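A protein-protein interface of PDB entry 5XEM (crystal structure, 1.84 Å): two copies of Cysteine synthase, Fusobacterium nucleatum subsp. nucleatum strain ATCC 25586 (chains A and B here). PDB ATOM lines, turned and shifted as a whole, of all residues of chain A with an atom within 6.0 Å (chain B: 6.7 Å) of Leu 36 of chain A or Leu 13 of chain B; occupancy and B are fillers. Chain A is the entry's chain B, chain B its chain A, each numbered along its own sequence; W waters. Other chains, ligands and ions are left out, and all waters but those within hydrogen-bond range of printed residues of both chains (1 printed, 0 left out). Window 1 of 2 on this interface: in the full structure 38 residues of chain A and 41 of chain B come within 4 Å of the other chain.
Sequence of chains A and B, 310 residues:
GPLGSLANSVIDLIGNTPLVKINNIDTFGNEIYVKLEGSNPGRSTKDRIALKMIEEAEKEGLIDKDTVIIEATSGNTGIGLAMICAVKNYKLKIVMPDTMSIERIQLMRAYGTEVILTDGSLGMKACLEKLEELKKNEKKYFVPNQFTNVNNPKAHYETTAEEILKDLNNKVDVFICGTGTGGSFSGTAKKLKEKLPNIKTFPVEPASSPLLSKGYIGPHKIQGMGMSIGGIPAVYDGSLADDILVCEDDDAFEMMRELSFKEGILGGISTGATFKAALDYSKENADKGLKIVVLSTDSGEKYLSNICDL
Hydrophobic or aromatic side chains of chain B that line the printed part of chain A: Leu 6, Ala 7, Val 10 and Leu 13. Of the 14 printed residues of chain A, 6 touch a printed residue of chain B. Printed residues of chain A that touch a printed residue of chain B: Thr 17, Pro 18, Leu 19, Val 20, Leu 36 and Ile 265. Hydrophobic or aromatic side chains of chain A within 4 Å of the printed part of chain B: Pro 18, Leu 19, Val 20, Leu 36 and Ile 265. Among the printed residues, no Asp or Glu carboxylate lies within 4 Å of a Lys or Arg side-chain nitrogen of the other chain.
Water W1 lies within hydrogen-bond range of the backbone carbonyl oxygen (O) of Ser 39 of chain A and the backbone carbonyl oxygen (O) of Ser 39 of chain B.
The backbone carbonyl oxygen (O) of Val 20 of chain A sits at hydrogen-bond distance from the backbone NH (N) of Val 34 of chain A, 2.7 Å away. The backbone carbonyl oxygen (O) of Pro 18 of chain A is in hydrogen-bond range of the backbone NH (N) of Leu 36 of chain A (2.9 Å). The side-chain hydroxyl (OG) of Ser 9 of chain B sits close to the backbone NH (N) of Ile 11 of chain B (3.1 Å). The backbone NH (N) of Ser 9 of chain B sits at hydrogen-bond distance from the side-chain carboxylate (OD2) of Asp 12 of chain B, 3.0 Å away. The side-chain amino group of Lys 35 of chain A lies within hydrogen-bond range of the side-chain hydroxyl of Thr 17 of chain A, at 2.9 Å. The side-chain carboxylate (OE2) of Glu 37 of chain A lies within hydrogen-bond range of the side-chain hydroxyl (OG1) of Thr 17 of chain A (2.6 Å).
Leu 13 of chain B touches just these residues of chain A: Pro 18 and Leu 36. Printed residues of chain B within 4 Å of Pro 18 of chain A: Ser 5 (3.3 Å) and Leu 13 (3.4 Å). Printed residues of chain A within 4 Å of Leu 6 of chain B: Leu 19. Of the printed residues of chain A, Ser 5 of chain B touches Thr 17 (3.8 Å), Pro 18 (3.3 Å) and Leu 19 (2.8 Å). Printed residues of chain B within 4 Å of Val 20 of chain A: Ala 7, Ser 9 and Val 10. Of the printed residues of chain B, Thr 17 of chain A touches Ser 5. Gly 15 of chain B touches none of the printed residues of chain A. The nearest printed residue of chain B that does not touch Pro 18 of chain A is Ala 7 of chain B (5.1 Å).
Ser 5 of chain B touches Thr 17 of chain A (CB to O, 3.8 Å). Pro 18 of chain A touches Ser 5 of chain B. CB of Pro 18 of chain A touches CD2 of Leu 13 of chain B, 3.4 Å away. CA of Leu 6 of chain B touches O of Leu 19 of chain A, at 3.4 Å. CA of Val 20 of chain A touches O of Ala 7 of chain B (3.3 Å). CG1 of Val 20 of chain A touches CA of Ser 9 of chain B, at 3.7 Å. Val 20 of chain A touches Val 10 of chain B (CG1 to N, 3.9 Å). Leu 13 of chain B touches Leu 36 of chain A. CG1 of Ile 265 of chain A touches CG1 of Val 10 of chain B (3.9 Å).
The backbone NH (N) of Ala 7 of chain B lies within hydrogen-bond range of the backbone carbonyl oxygen (O) of Leu 19 of chain A (2.6 Å). O of Ser 5 of chain B sits at hydrogen-bond distance from N of Leu 19 of chain A (2.8 Å).
Positions printed for both chains: 17, 39 and 40. Of the 11 pairs that touch across the chains among the printed residues, none has its exchanged pair printed and touching as well.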
ATOM      1  N   THR A  17      -8.318  31.466 -14.583  1.00  0.00           N
ATOM      2  CA  THR A  17      -7.129  30.821 -15.121  1.00  0.00           C
ATOM      3  C   THR A  17      -7.323  29.321 -15.184  1.00  0.00           C
ATOM      4  O   THR A  17      -8.167  28.759 -14.464  1.00  0.00           O
ATOM      5  CB  THR A  17      -5.926  31.121 -14.233  1.00  0.00           C
ATOM      6  OG1 THR A  17      -6.246  30.729 -12.895  1.00  0.00           O
ATOM      7  CG2 THR A  17      -5.576  32.639 -14.280  1.00  0.00           C
ATOM      8  N   PRO A  18      -6.540  28.660 -16.036  1.00  0.00           N
ATOM      9  CA  PRO A  18      -6.804  27.242 -16.181  1.00  0.00           C
ATOM     10  C   PRO A  18      -6.230  26.389 -15.065  1.00  0.00           C
ATOM     11  O   PRO A  18      -5.279  26.772 -14.375  1.00  0.00           O
ATOM     12  CB  PRO A  18      -6.127  26.891 -17.501  1.00  0.00           C
ATOM     13  CG  PRO A  18      -5.056  27.877 -17.669  1.00  0.00           C
ATOM     14  CD  PRO A  18      -5.490  29.137 -16.958  1.00  0.00           C
ATOM     15  N   LEU A  19      -6.853  25.232 -14.894  1.00  0.00           N
ATOM     16  CA  LEU A  19      -6.411  24.275 -13.928  1.00  0.00           C
ATOM     17  C   LEU A  19      -6.040  23.044 -14.790  1.00  0.00           C
ATOM     18  O   LEU A  19      -6.830  22.596 -15.589  1.00  0.00           O
ATOM     19  CB  LEU A  19      -7.570  24.095 -12.945  1.00  0.00           C
ATOM     20  CG  LEU A  19      -7.360  23.201 -11.763  1.00  0.00           C
ATOM     21  CD1 LEU A  19      -6.201  23.656 -10.892  1.00  0.00           C
ATOM     22  CD2 LEU A  19      -8.671  23.057 -10.979  1.00  0.00           C
ATOM     23  N   VAL A  20      -4.797  22.595 -14.735  1.00  0.00           N
ATOM     24  CA  VAL A  20      -4.295  21.571 -15.639  1.00  0.00           C
ATOM     25  C   VAL A  20      -3.903  20.309 -14.845  1.00  0.00           C
ATOM     26  O   VAL A  20      -3.211  20.412 -13.814  1.00  0.00           O
ATOM     27  CB  VAL A  20      -3.045  22.082 -16.384  1.00  0.00           C
ATOM     28  CG1 VAL A  20      -2.567  21.018 -17.357  1.00  0.00           C
ATOM     29  CG2 VAL A  20      -3.350  23.408 -17.108  1.00  0.00           C
ATOM     30  N   VAL A  34      -2.633  21.743 -11.493  1.00  0.00           N
ATOM     31  CA  VAL A  34      -1.831  22.938 -11.297  1.00  0.00           C
ATOM     32  C   VAL A  34      -2.656  24.112 -11.799  1.00  0.00           C
ATOM     33  O   VAL A  34      -3.090  24.102 -12.910  1.00  0.00           O
ATOM     34  CB  VAL A  34      -0.482  22.861 -12.024  1.00  0.00           C
ATOM     35  CG1 VAL A  34       0.311  24.151 -11.824  1.00  0.00           C
ATOM     36  CG2 VAL A  34       0.317  21.664 -11.520  1.00  0.00           C
ATOM     37  N   LYS A  35      -2.896  25.088 -10.932  1.00  0.00           N
ATOM     38  CA  LYS A  35      -3.657  26.270 -11.342  1.00  0.00           C
ATOM     39  C   LYS A  35      -2.679  27.297 -11.914  1.00  0.00           C
ATOM     40  O   LYS A  35      -1.812  27.741 -11.202  1.00  0.00           O
ATOM     41  CB  LYS A  35      -4.411  26.871 -10.175  1.00  0.00           C
ATOM     42  CG  LYS A  35      -5.326  28.013 -10.656  1.00  0.00           C
ATOM     43  CD  LYS A  35      -6.469  28.243  -9.723  1.00  0.00           C
ATOM     44  CE  LYS A  35      -7.363  29.386 -10.177  1.00  0.00           C
ATOM     45  NZ  LYS A  35      -8.152  29.094 -11.387  1.00  0.00           N
ATOM     46  N   LEU A  36      -2.785  27.606 -13.206  1.00  0.00           N
ATOM     47  CA  LEU A  36      -1.714  28.310 -13.921  1.00  0.00           C
ATOM     48  C   LEU A  36      -1.969  29.809 -13.892  1.00  0.00           C
ATOM     49  O   LEU A  36      -2.558  30.360 -14.807  1.00  0.00           O
ATOM     50  CB  LEU A  36      -1.552  27.828 -15.372  1.00  0.00           C
ATOM     51  CG  LEU A  36      -1.109  26.383 -15.562  1.00  0.00           C
ATOM     52  CD1 LEU A  36      -1.128  26.014 -17.039  1.00  0.00           C
ATOM     53  CD2 LEU A  36       0.278  26.173 -14.963  1.00  0.00           C
ATOM     54  N   GLU A  37      -1.474  30.449 -12.835  1.00  0.00           N
ATOM     55  CA  GLU A  37      -1.635  31.909 -12.676  1.00  0.00           C
ATOM     56  C   GLU A  37      -0.725  32.700 -13.588  1.00  0.00           C
ATOM     57  O   GLU A  37      -0.926  33.901 -13.761  1.00  0.00           O
ATOM     58  CB  GLU A  37      -1.460  32.320 -11.232  1.00  0.00           C
ATOM     59  CG  GLU A  37      -2.499  31.728 -10.300  1.00  0.00           C
ATOM     60  CD  GLU A  37      -3.865  32.344 -10.505  1.00  0.00           C
ATOM     61  OE1 GLU A  37      -4.002  33.571 -10.294  1.00  0.00           O
ATOM     62  OE2 GLU A  37      -4.798  31.605 -10.863  1.00  0.00           O
ATOM     63  N   GLY A  38       0.263  32.031 -14.184  1.00  0.00           N
ATOM     64  CA  GLY A  38       1.034  32.609 -15.261  1.00  0.00           C
ATOM     65  C   GLY A  38       0.211  32.923 -16.486  1.00  0.00           C
ATOM     66  O   GLY A  38       0.681  33.636 -17.358  1.00  0.00           O
ATOM     67  N   SER A  39      -1.015  32.406 -16.555  1.00  0.00           N
ATOM     68  CA  SER A  39      -1.919  32.682 -17.653  1.00  0.00           C
ATOM     69  C   SER A  39      -2.576  34.034 -17.572  1.00  0.00           C
ATOM     70  O   SER A  39      -3.162  34.504 -18.563  1.00  0.00           O
ATOM     71  CB  SER A  39      -3.010  31.609 -17.732  1.00  0.00           C
ATOM     72  OG  SER A  39      -2.385  30.401 -18.104  1.00  0.00           O
ATOM     73  N   ASN A  40      -2.517  34.656 -16.396  1.00  0.00           N
ATOM     74  CA  ASN A  40      -2.986  36.039 -16.243  1.00  0.00           C
ATOM     75  C   ASN A  40      -2.213  36.957 -17.206  1.00  0.00           C
ATOM     76  O   ASN A  40      -1.066  36.690 -17.526  1.00  0.00           O
ATOM     77  CB  ASN A  40      -2.802  36.528 -14.809  1.00  0.00           C
ATOM     78  CG  ASN A  40      -3.875  36.017 -13.868  1.00  0.00           C
ATOM     79  OD1 ASN A  40      -5.037  36.373 -13.997  1.00  0.00           O
ATOM     80  ND2 ASN A  40      -3.483  35.184 -12.911  1.00  0.00           N
ATOM     81  N   ILE A 265       4.533  22.562 -19.016  1.00  0.00           N
ATOM     82  CA  ILE A 265       4.149  23.635 -18.085  1.00  0.00           C
ATOM     83  C   ILE A 265       5.419  24.416 -17.752  1.00  0.00           C
ATOM     84  O   ILE A 265       6.361  23.872 -17.169  1.00  0.00           O
ATOM     85  CB  ILE A 265       3.567  23.070 -16.765  1.00  0.00           C
ATOM     86  CG1 ILE A 265       2.256  22.345 -17.016  1.00  0.00           C
ATOM     87  CG2 ILE A 265       3.351  24.193 -15.762  1.00  0.00           C
ATOM     88  CD1 ILE A 265       1.662  21.618 -15.783  1.00  0.00           C
ATOM     89  N   VAL A 294      -2.295  22.601  -6.793  1.00  0.00           N
ATOM     90  CA  VAL A 294      -1.068  23.338  -6.571  1.00  0.00           C
ATOM     91  C   VAL A 294      -1.243  24.698  -7.268  1.00  0.00           C
ATOM     92  O   VAL A 294      -1.561  24.727  -8.450  1.00  0.00           O
ATOM     93  CB  VAL A 294       0.135  22.587  -7.203  1.00  0.00           C
ATOM     94  CG1 VAL A 294       1.392  23.461  -7.241  1.00  0.00           C
ATOM     95  CG2 VAL A 294       0.418  21.253  -6.489  1.00  0.00           C
ATOM     96  N   SER A 296       0.343  27.647  -9.139  1.00  0.00           N
ATOM     97  CA  SER A 296       1.560  28.101  -9.824  1.00  0.00           C
ATOM     98  C   SER A 296       1.454  29.613  -9.909  1.00  0.00           C
ATOM     99  O   SER A 296       0.620  30.121 -10.652  1.00  0.00           O
ATOM    100  CB  SER A 296       1.663  27.524 -11.223  1.00  0.00           C
ATOM    101  OG  SER A 296       2.707  28.129 -11.981  1.00  0.00           O
ATOM    102  N   SER B   5     -12.533  26.096 -16.387  1.00  0.00           N
ATOM    103  CA  SER B   5     -11.249  25.970 -17.141  1.00  0.00           C
ATOM    104  C   SER B   5     -10.371  24.805 -16.628  1.00  0.00           C
ATOM    105  O   SER B   5      -9.140  24.950 -16.555  1.00  0.00           O
ATOM    106  CB  SER B   5     -10.469  27.289 -17.079  1.00  0.00           C
ATOM    107  OG  SER B   5     -11.224  28.348 -17.630  1.00  0.00           O
ATOM    108  N   LEU B   6     -10.990  23.655 -16.291  1.00  0.00           N
ATOM    109  CA  LEU B   6     -10.209  22.429 -16.029  1.00  0.00           C
ATOM    110  C   LEU B   6      -9.663  21.875 -17.352  1.00  0.00           C
ATOM    111  O   LEU B   6     -10.438  21.673 -18.294  1.00  0.00           O
ATOM    112  CB  LEU B   6     -11.038  21.364 -15.325  1.00  0.00           C
ATOM    113  CG  LEU B   6     -10.262  20.155 -14.783  1.00  0.00           C
ATOM    114  CD1 LEU B   6      -9.293  20.592 -13.713  1.00  0.00           C
ATOM    115  CD2 LEU B   6     -11.186  19.114 -14.197  1.00  0.00           C
ATOM    116  N   ALA B   7      -8.350  21.637 -17.429  1.00  0.00           N
ATOM    117  CA  ALA B   7      -7.720  21.117 -18.655  1.00  0.00           C
ATOM    118  C   ALA B   7      -7.004  19.804 -18.367  1.00  0.00           C
ATOM    119  O   ALA B   7      -6.369  19.643 -17.313  1.00  0.00           O
ATOM    120  CB  ALA B   7      -6.708  22.113 -19.210  1.00  0.00           C
ATOM    121  N   SER B   9      -4.481  18.692 -20.351  1.00  0.00           N
ATOM    122  CA  SER B   9      -3.087  19.089 -20.502  1.00  0.00           C
ATOM    123  C   SER B   9      -3.053  20.495 -21.065  1.00  0.00           C
ATOM    124  O   SER B   9      -4.089  21.074 -21.432  1.00  0.00           O
ATOM    125  CB  SER B   9      -2.348  18.149 -21.454  1.00  0.00           C
ATOM    126  OG  SER B   9      -2.743  18.441 -22.796  1.00  0.00           O
ATOM    127  N   VAL B  10      -1.849  21.042 -21.151  1.00  0.00           N
ATOM    128  CA  VAL B  10      -1.703  22.384 -21.748  1.00  0.00           C
ATOM    129  C   VAL B  10      -2.207  22.443 -23.199  1.00  0.00           C
ATOM    130  O   VAL B  10      -2.577  23.503 -23.703  1.00  0.00           O
ATOM    131  CB  VAL B  10      -0.258  22.925 -21.637  1.00  0.00           C
ATOM    132  CG1 VAL B  10       0.124  23.170 -20.165  1.00  0.00           C
ATOM    133  CG2 VAL B  10       0.750  22.020 -22.332  1.00  0.00           C
ATOM    134  N   ILE B  11      -2.222  21.304 -23.888  1.00  0.00           N
ATOM    135  CA  ILE B  11      -2.788  21.277 -25.243  1.00  0.00           C
ATOM    136  C   ILE B  11      -4.209  21.797 -25.274  1.00  0.00           C
ATOM    137  O   ILE B  11      -4.627  22.437 -26.242  1.00  0.00           O
ATOM    138  CB  ILE B  11      -2.751  19.850 -25.853  1.00  0.00           C
ATOM    139  CG1 ILE B  11      -1.290  19.412 -25.998  1.00  0.00           C
ATOM    140  CG2 ILE B  11      -3.563  19.814 -27.172  1.00  0.00           C
ATOM    141  CD1 ILE B  11      -1.072  17.992 -26.529  1.00  0.00           C
ATOM    142  N   ASP B  12      -4.969  21.548 -24.208  1.00  0.00           N
ATOM    143  CA  ASP B  12      -6.352  22.003 -24.175  1.00  0.00           C
ATOM    144  C   ASP B  12      -6.504  23.521 -24.008  1.00  0.00           C
ATOM    145  O   ASP B  12      -7.589  24.069 -24.210  1.00  0.00           O
ATOM    146  CB  ASP B  12      -7.146  21.268 -23.077  1.00  0.00           C
ATOM    147  CG  ASP B  12      -7.146  19.770 -23.276  1.00  0.00           C
ATOM    148  OD1 ASP B  12      -7.570  19.297 -24.351  1.00  0.00           O
ATOM    149  OD2 ASP B  12      -6.675  19.060 -22.384  1.00  0.00           O
ATOM    150  N   LEU B  13      -5.429  24.219 -23.656  1.00  0.00           N
ATOM    151  CA  LEU B  13      -5.472  25.673 -23.539  1.00  0.00           C
ATOM    152  C   LEU B  13      -5.226  26.427 -24.860  1.00  0.00           C
ATOM    153  O   LEU B  13      -5.291  27.653 -24.893  1.00  0.00           O
ATOM    154  CB  LEU B  13      -4.460  26.147 -22.509  1.00  0.00           C
ATOM    155  CG  LEU B  13      -4.501  25.433 -21.146  1.00  0.00           C
ATOM    156  CD1 LEU B  13      -3.468  26.038 -20.195  1.00  0.00           C
ATOM    157  CD2 LEU B  13      -5.899  25.453 -20.577  1.00  0.00           C
ATOM    158  N   ILE B  14      -4.908  25.698 -25.922  1.00  0.00           N
ATOM    159  CA  ILE B  14      -4.605  26.277 -27.226  1.00  0.00           C
ATOM    160  C   ILE B  14      -5.916  26.791 -27.819  1.00  0.00           C
ATOM    161  O   ILE B  14      -6.943  26.096 -27.795  1.00  0.00           O
ATOM    162  CB  ILE B  14      -3.921  25.262 -28.168  1.00  0.00           C
ATOM    163  CG1 ILE B  14      -2.549  24.866 -27.593  1.00  0.00           C
ATOM    164  CG2 ILE B  14      -3.739  25.838 -29.590  1.00  0.00           C
ATOM    165  CD1 ILE B  14      -1.854  23.700 -28.310  1.00  0.00           C
ATOM    166  N   GLY B  15      -5.869  28.007 -28.341  1.00  0.00           N
ATOM    167  CA  GLY B  15      -7.000  28.627 -28.989  1.00  0.00           C
ATOM    168  C   GLY B  15      -7.947  29.301 -28.029  1.00  0.00           C
ATOM    169  O   GLY B  15      -7.656  29.470 -26.854  1.00  0.00           O
ATOM    170  N   ASN B  16      -9.093  29.716 -28.544  1.00  0.00           N
ATOM    171  CA  ASN B  16     -10.050  30.496 -27.775  1.00  0.00           C
ATOM    172  C   ASN B  16      -9.423  31.694 -27.070  1.00  0.00           C
ATOM    173  O   ASN B  16      -9.588  31.929 -25.871  1.00  0.00           O
ATOM    174  CB  ASN B  16     -10.811  29.582 -26.832  1.00  0.00           C
ATOM    175  CG  ASN B  16     -11.667  28.613 -27.605  1.00  0.00           C
ATOM    176  OD1 ASN B  16     -12.564  29.028 -28.332  1.00  0.00           O
ATOM    177  ND2 ASN B  16     -11.324  27.351 -27.558  1.00  0.00           N
ATOM    178  N   THR B  17      -8.663  32.438 -27.843  1.00  0.00           N
ATOM    179  CA  THR B  17      -7.923  33.577 -27.330  1.00  0.00           C
ATOM    180  C   THR B  17      -8.817  34.804 -27.305  1.00  0.00           C
ATOM    181  O   THR B  17      -9.741  34.912 -28.097  1.00  0.00           O
ATOM    182  CB  THR B  17      -6.707  33.894 -28.203  1.00  0.00           C
ATOM    183  OG1 THR B  17      -7.127  34.050 -29.560  1.00  0.00           O
ATOM    184  CG2 THR B  17      -5.692  32.718 -28.112  1.00  0.00           C
ATOM    185  N   SER B  39      -1.908  34.791 -25.608  1.00  0.00           N
ATOM    186  CA  SER B  39      -2.623  34.108 -24.540  1.00  0.00           C
ATOM    187  C   SER B  39      -2.525  32.595 -24.663  1.00  0.00           C
ATOM    188  O   SER B  39      -2.817  31.890 -23.693  1.00  0.00           O
ATOM    189  CB  SER B  39      -4.092  34.499 -24.529  1.00  0.00           C
ATOM    190  OG  SER B  39      -4.211  35.888 -24.241  1.00  0.00           O
ATOM    191  N   ASN B  40      -2.161  32.088 -25.850  1.00  0.00           N
ATOM    192  CA  ASN B  40      -1.885  30.660 -26.010  1.00  0.00           C
ATOM    193  C   ASN B  40      -0.820  30.194 -24.996  1.00  0.00           C
ATOM    194  O   ASN B  40       0.039  30.987 -24.584  1.00  0.00           O
ATOM    195  CB  ASN B  40      -1.421  30.336 -27.438  1.00  0.00           C
ATOM    196  CG  ASN B  40      -2.554  30.365 -28.453  1.00  0.00           C
ATOM    197  OD1 ASN B  40      -2.555  31.193 -29.365  1.00  0.00           O
ATOM    198  ND2 ASN B  40      -3.523  29.502 -28.285  1.00  0.00           N
ATOM    199  N   PRO B  41      -0.858  28.904 -24.587  1.00  0.00           N
ATOM    200  CA  PRO B  41       0.085  28.443 -23.536  1.00  0.00           C
ATOM    201  C   PRO B  41       1.567  28.518 -23.954  1.00  0.00           C
ATOM    202  O   PRO B  41       2.461  28.764 -23.105  1.00  0.00           O
ATOM    203  CB  PRO B  41      -0.389  26.989 -23.261  1.00  0.00           C
ATOM    204  CG  PRO B  41      -1.129  26.603 -24.504  1.00  0.00           C
ATOM    205  CD  PRO B  41      -1.839  27.855 -24.919  1.00  0.00           C
ATOM    206  N   ASP B  47       1.157  27.770 -31.619  1.00  0.00           N
ATOM    207  CA  ASP B  47       0.614  26.633 -30.900  1.00  0.00           C
ATOM    208  C   ASP B  47      -0.503  25.969 -31.756  1.00  0.00           C
ATOM    209  O   ASP B  47      -0.645  24.726 -31.771  1.00  0.00           O
ATOM    210  CB  ASP B  47      -0.057  27.087 -29.600  1.00  0.00           C
ATOM    211  CG  ASP B  47       0.897  27.428 -28.482  1.00  0.00           C
ATOM    212  OD1 ASP B  47       2.126  27.505 -28.725  1.00  0.00           O
ATOM    213  OD2 ASP B  47       0.391  27.633 -27.338  1.00  0.00           O
HETATM  214  O   HOH W   1      -2.855  33.541 -21.093  1.00  0.00           O
